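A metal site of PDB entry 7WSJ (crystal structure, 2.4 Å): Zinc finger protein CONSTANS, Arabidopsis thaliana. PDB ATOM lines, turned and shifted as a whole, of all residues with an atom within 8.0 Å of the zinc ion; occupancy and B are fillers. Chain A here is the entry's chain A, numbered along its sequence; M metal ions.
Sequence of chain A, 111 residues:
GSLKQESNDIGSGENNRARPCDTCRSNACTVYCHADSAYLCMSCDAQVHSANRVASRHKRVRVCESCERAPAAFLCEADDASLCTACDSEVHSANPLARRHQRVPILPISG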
ATOM      1  N   TYR A  32      28.182 -31.766   3.071  1.00  0.00           N
ATOM      2  CA  TYR A  32      28.561 -30.606   2.284  1.00  0.00           C
ATOM      3  C   TYR A  32      27.303 -29.801   2.000  1.00  0.00           C
ATOM      4  O   TYR A  32      26.265 -30.381   1.633  1.00  0.00           O
ATOM      5  CB  TYR A  32      29.258 -30.994   0.984  1.00  0.00           C
ATOM      6  CG  TYR A  32      29.488 -29.830   0.047  1.00  0.00           C
ATOM      7  CD1 TYR A  32      30.500 -28.904   0.289  1.00  0.00           C
ATOM      8  CD2 TYR A  32      28.706 -29.650  -1.089  1.00  0.00           C
ATOM      9  CE1 TYR A  32      30.714 -27.842  -0.562  1.00  0.00           C
ATOM     10  CE2 TYR A  32      28.917 -28.586  -1.954  1.00  0.00           C
ATOM     11  CZ  TYR A  32      29.924 -27.683  -1.677  1.00  0.00           C
ATOM     12  OH  TYR A  32      30.143 -26.629  -2.529  1.00  0.00           O
ATOM     13  N   CYS A  33      27.404 -28.491   2.163  1.00  0.00           N
ATOM     14  CA  CYS A  33      26.335 -27.553   1.849  1.00  0.00           C
ATOM     15  C   CYS A  33      26.846 -26.625   0.756  1.00  0.00           C
ATOM     16  O   CYS A  33      27.788 -25.857   0.982  1.00  0.00           O
ATOM     17  CB  CYS A  33      25.894 -26.770   3.088  1.00  0.00           C
ATOM     18  SG  CYS A  33      24.565 -25.601   2.742  1.00  0.00           S
ATOM     19  N   HIS A  34      26.225 -26.719  -0.419  1.00  0.00           N
ATOM     20  CA  HIS A  34      26.622 -25.898  -1.551  1.00  0.00           C
ATOM     21  C   HIS A  34      26.231 -24.443  -1.345  1.00  0.00           C
ATOM     22  O   HIS A  34      26.967 -23.537  -1.746  1.00  0.00           O
ATOM     23  CB  HIS A  34      26.000 -26.460  -2.820  1.00  0.00           C
ATOM     24  CG  HIS A  34      26.637 -25.965  -4.078  1.00  0.00           C
ATOM     25  ND1 HIS A  34      27.995 -26.011  -4.292  1.00  0.00           N
ATOM     26  CD2 HIS A  34      26.102 -25.425  -5.196  1.00  0.00           C
ATOM     27  CE1 HIS A  34      28.273 -25.521  -5.493  1.00  0.00           C
ATOM     28  NE2 HIS A  34      27.141 -25.147  -6.058  1.00  0.00           N
ATOM     29  N   ALA A  35      25.075 -24.203  -0.716  1.00  0.00           N
ATOM     30  CA  ALA A  35      24.646 -22.839  -0.469  1.00  0.00           C
ATOM     31  C   ALA A  35      25.653 -22.100   0.415  1.00  0.00           C
ATOM     32  O   ALA A  35      25.967 -20.935   0.164  1.00  0.00           O
ATOM     33  CB  ALA A  35      23.258 -22.826   0.176  1.00  0.00           C
ATOM     34  N   ASP A  36      26.183 -22.773   1.425  1.00  0.00           N
ATOM     35  CA  ASP A  36      27.201 -22.188   2.290  1.00  0.00           C
ATOM     36  C   ASP A  36      28.619 -22.462   1.822  1.00  0.00           C
ATOM     37  O   ASP A  36      29.554 -21.925   2.415  1.00  0.00           O
ATOM     38  CB  ASP A  36      27.041 -22.709   3.725  1.00  0.00           C
ATOM     39  CG  ASP A  36      25.863 -22.097   4.442  1.00  0.00           C
ATOM     40  OD1 ASP A  36      25.651 -20.867   4.282  1.00  0.00           O
ATOM     41  OD2 ASP A  36      25.155 -22.821   5.160  1.00  0.00           O
ATOM     42  N   SER A  37      28.802 -23.265   0.770  1.00  0.00           N
ATOM     43  CA  SER A  37      30.128 -23.638   0.281  1.00  0.00           C
ATOM     44  C   SER A  37      30.980 -24.193   1.420  1.00  0.00           C
ATOM     45  O   SER A  37      32.135 -23.791   1.621  1.00  0.00           O
ATOM     46  CB  SER A  37      30.818 -22.449  -0.384  1.00  0.00           C
ATOM     47  OG  SER A  37      29.978 -21.802  -1.320  1.00  0.00           O
ATOM     48  N   ALA A  38      30.396 -25.115   2.187  1.00  0.00           N
ATOM     49  CA  ALA A  38      31.020 -25.513   3.440  1.00  0.00           C
ATOM     50  C   ALA A  38      30.898 -27.010   3.675  1.00  0.00           C
ATOM     51  O   ALA A  38      29.834 -27.600   3.443  1.00  0.00           O
ATOM     52  CB  ALA A  38      30.402 -24.767   4.631  1.00  0.00           C
ATOM     53  N   LEU A  40      30.830 -29.698   6.702  1.00  0.00           N
ATOM     54  CA  LEU A  40      30.434 -29.615   8.104  1.00  0.00           C
ATOM     55  C   LEU A  40      30.318 -31.016   8.710  1.00  0.00           C
ATOM     56  O   LEU A  40      29.927 -31.965   8.028  1.00  0.00           O
ATOM     57  CB  LEU A  40      29.080 -28.898   8.258  1.00  0.00           C
ATOM     58  CG  LEU A  40      28.961 -27.474   7.709  1.00  0.00           C
ATOM     59  CD1 LEU A  40      27.521 -26.995   7.791  1.00  0.00           C
ATOM     60  CD2 LEU A  40      29.886 -26.540   8.463  1.00  0.00           C
ATOM     61  N   ASP A  45      26.527 -28.969  11.393  1.00  0.00           N
ATOM     62  CA  ASP A  45      25.410 -28.919  10.464  1.00  0.00           C
ATOM     63  C   ASP A  45      24.122 -28.518  11.188  1.00  0.00           C
ATOM     64  O   ASP A  45      23.404 -27.613  10.748  1.00  0.00           O
ATOM     65  CB  ASP A  45      25.241 -30.270   9.781  1.00  0.00           C
ATOM     66  CG  ASP A  45      24.159 -30.259   8.746  1.00  0.00           C
ATOM     67  OD1 ASP A  45      24.249 -29.413   7.839  1.00  0.00           O
ATOM     68  OD2 ASP A  45      23.226 -31.081   8.832  1.00  0.00           O
ATOM     69  N   VAL A  48      24.329 -24.833  12.337  1.00  0.00           N
ATOM     70  CA  VAL A  48      24.237 -23.837  11.280  1.00  0.00           C
ATOM     71  C   VAL A  48      22.822 -23.757  10.726  1.00  0.00           C
ATOM     72  O   VAL A  48      22.300 -22.657  10.477  1.00  0.00           O
ATOM     73  CB  VAL A  48      25.261 -24.156  10.176  1.00  0.00           C
ATOM     74  CG1 VAL A  48      24.930 -23.374   8.904  1.00  0.00           C
ATOM     75  CG2 VAL A  48      26.662 -23.833  10.645  1.00  0.00           C
ATOM     76  N   HIS A  49      22.168 -24.899  10.504  1.00  0.00           N
ATOM     77  CA  HIS A  49      20.913 -24.870   9.767  1.00  0.00           C
ATOM     78  C   HIS A  49      19.676 -24.871  10.663  1.00  0.00           C
ATOM     79  O   HIS A  49      18.560 -24.724  10.143  1.00  0.00           O
ATOM     80  CB  HIS A  49      20.862 -26.033   8.783  1.00  0.00           C
ATOM     81  CG  HIS A  49      21.987 -26.008   7.797  1.00  0.00           C
ATOM     82  ND1 HIS A  49      23.152 -26.715   7.979  1.00  0.00           N
ATOM     83  CD2 HIS A  49      22.135 -25.332   6.642  1.00  0.00           C
ATOM     84  CE1 HIS A  49      23.971 -26.478   6.975  1.00  0.00           C
ATOM     85  NE2 HIS A  49      23.379 -25.644   6.139  1.00  0.00           N
ATOM     86  N   VAL A  54      15.310 -19.680   7.306  1.00  0.00           N
ATOM     87  CA  VAL A  54      15.967 -19.499   6.017  1.00  0.00           C
ATOM     88  C   VAL A  54      17.087 -20.518   5.834  1.00  0.00           C
ATOM     89  O   VAL A  54      17.182 -21.190   4.807  1.00  0.00           O
ATOM     90  CB  VAL A  54      16.488 -18.055   5.870  1.00  0.00           C
ATOM     91  CG1 VAL A  54      17.247 -17.893   4.566  1.00  0.00           C
ATOM     92  CG2 VAL A  54      15.329 -17.067   5.934  1.00  0.00           C
ATOM     93  N   ALA A  55      17.943 -20.653   6.858  1.00  0.00           N
ATOM     94  CA  ALA A  55      19.069 -21.569   6.764  1.00  0.00           C
ATOM     95  C   ALA A  55      18.611 -23.025   6.760  1.00  0.00           C
ATOM     96  O   ALA A  55      19.290 -23.885   6.175  1.00  0.00           O
ATOM     97  CB  ALA A  55      20.046 -21.325   7.913  1.00  0.00           C
ATOM     98  N   SER A  56      17.477 -23.321   7.400  1.00  0.00           N
ATOM     99  CA  SER A  56      17.000 -24.695   7.458  1.00  0.00           C
ATOM    100  C   SER A  56      16.596 -25.235   6.097  1.00  0.00           C
ATOM    101  O   SER A  56      16.478 -26.462   5.946  1.00  0.00           O
ATOM    102  CB  SER A  56      15.820 -24.808   8.425  1.00  0.00           C
ATOM    103  OG  SER A  56      14.705 -24.055   7.962  1.00  0.00           O
ATOM    104  N   ARG A  57      16.381 -24.376   5.108  1.00  0.00           N
ATOM    105  CA  ARG A  57      15.998 -24.826   3.774  1.00  0.00           C
ATOM    106  C   ARG A  57      17.184 -25.301   2.946  1.00  0.00           C
ATOM    107  O   ARG A  57      16.975 -25.912   1.893  1.00  0.00           O
ATOM    108  CB  ARG A  57      15.273 -23.711   3.024  1.00  0.00           C
ATOM    109  CG  ARG A  57      14.137 -23.074   3.793  1.00  0.00           C
ATOM    110  CD  ARG A  57      12.922 -23.976   3.848  1.00  0.00           C
ATOM    111  NE  ARG A  57      11.906 -23.462   4.747  1.00  0.00           N
ATOM    112  CZ  ARG A  57      11.780 -23.830   6.017  1.00  0.00           C
ATOM    113  NH1 ARG A  57      12.609 -24.733   6.536  1.00  0.00           N
ATOM    114  NH2 ARG A  57      10.824 -23.307   6.774  1.00  0.00           N
ATOM    115  N   HIS A  58      18.410 -25.016   3.381  1.00  0.00           N
ATOM    116  CA  HIS A  58      19.585 -25.393   2.618  1.00  0.00           C
ATOM    117  C   HIS A  58      19.620 -26.890   2.385  1.00  0.00           C
ATOM    118  O   HIS A  58      19.379 -27.686   3.299  1.00  0.00           O
ATOM    119  CB  HIS A  58      20.861 -24.953   3.342  1.00  0.00           C
ATOM    120  CG  HIS A  58      21.048 -23.472   3.397  1.00  0.00           C
ATOM    121  ND1 HIS A  58      22.150 -22.879   3.978  1.00  0.00           N
ATOM    122  CD2 HIS A  58      20.268 -22.459   2.945  1.00  0.00           C
ATOM    123  CE1 HIS A  58      22.038 -21.568   3.886  1.00  0.00           C
ATOM    124  NE2 HIS A  58      20.912 -21.283   3.259  1.00  0.00           N
ATOM    125  N   LYS A  59      19.910 -27.290   1.152  1.00  0.00           N
ATOM    126  CA  LYS A  59      20.044 -28.689   0.802  1.00  0.00           C
ATOM    127  C   LYS A  59      21.494 -29.128   0.984  1.00  0.00           C
ATOM    128  O   LYS A  59      22.413 -28.461   0.499  1.00  0.00           O
ATOM    129  CB  LYS A  59      19.592 -28.944  -0.628  1.00  0.00           C
ATOM    130  CG  LYS A  59      18.247 -28.333  -0.973  1.00  0.00           C
ATOM    131  CD  LYS A  59      17.634 -29.051  -2.159  1.00  0.00           C
ATOM    132  CE  LYS A  59      18.533 -28.988  -3.386  1.00  0.00           C
ATOM    133  NZ  LYS A  59      18.035 -29.877  -4.460  1.00  0.00           N
ATOM    134  N   ARG A  60      21.681 -30.245   1.675  1.00  0.00           N
ATOM    135  CA  ARG A  60      23.010 -30.742   1.999  1.00  0.00           C
ATOM    136  C   ARG A  60      23.120 -32.198   1.575  1.00  0.00           C
ATOM    137  O   ARG A  60      22.116 -32.910   1.463  1.00  0.00           O
ATOM    138  CB  ARG A  60      23.298 -30.612   3.493  1.00  0.00           C
ATOM    139  CG  ARG A  60      23.269 -29.186   3.999  1.00  0.00           C
ATOM    140  CD  ARG A  60      22.637 -29.127   5.352  1.00  0.00           C
ATOM    141  NE  ARG A  60      21.205 -28.862   5.300  1.00  0.00           N
ATOM    142  CZ  ARG A  60      20.382 -29.004   6.343  1.00  0.00           C
ATOM    143  NH1 ARG A  60      20.856 -29.424   7.508  1.00  0.00           N
ATOM    144  NH2 ARG A  60      19.098 -28.737   6.211  1.00  0.00           N
HETATM  145 ZN    ZN M   1      23.957 -24.204   4.450  1.00  0.00          ZN
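Four residues have an atom within 4 Å of the zinc ion: Cys 33, Asp 36, His 49 and His 58.
Along chain A the residues within 4 Å of the zinc ion span positions 33 to 58.
The nearest printed residue that does not touch the zinc ion is Ala 35 (4.5 Å).
The side-chain carboxylate (OD2) of Asp 36 binds the zinc ion (2.0 Å).
SG of Cys 33 is bound to the zinc ion.
The zinc ion is bound by ND1 of His 58, 2.3 Å away.
A ring nitrogen (NE2) of His 49 binds the zinc ion, 2.3 Å away.
The zinc ion has four donor atoms within binding distance.
The side-chain sulfur (SG) of Cys 33 lies close to the backbone NH (N) of Ala 35 (3.8 Å).
The backbone NH (N) of Cys 33 sits at hydrogen-bond distance from the backbone carbonyl oxygen (O) of Ala 38 (2.9 Å).
The backbone carbonyl oxygen (O) of His 58 is in hydrogen-bond range of the guanidinium group (NE) of Arg 60, at 3.0 Å.
ND1 of His 49 sits at hydrogen-bond distance from OD1 of Asp 45 (2.9 Å).
N of Ser 56 sits close to O of His 49.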
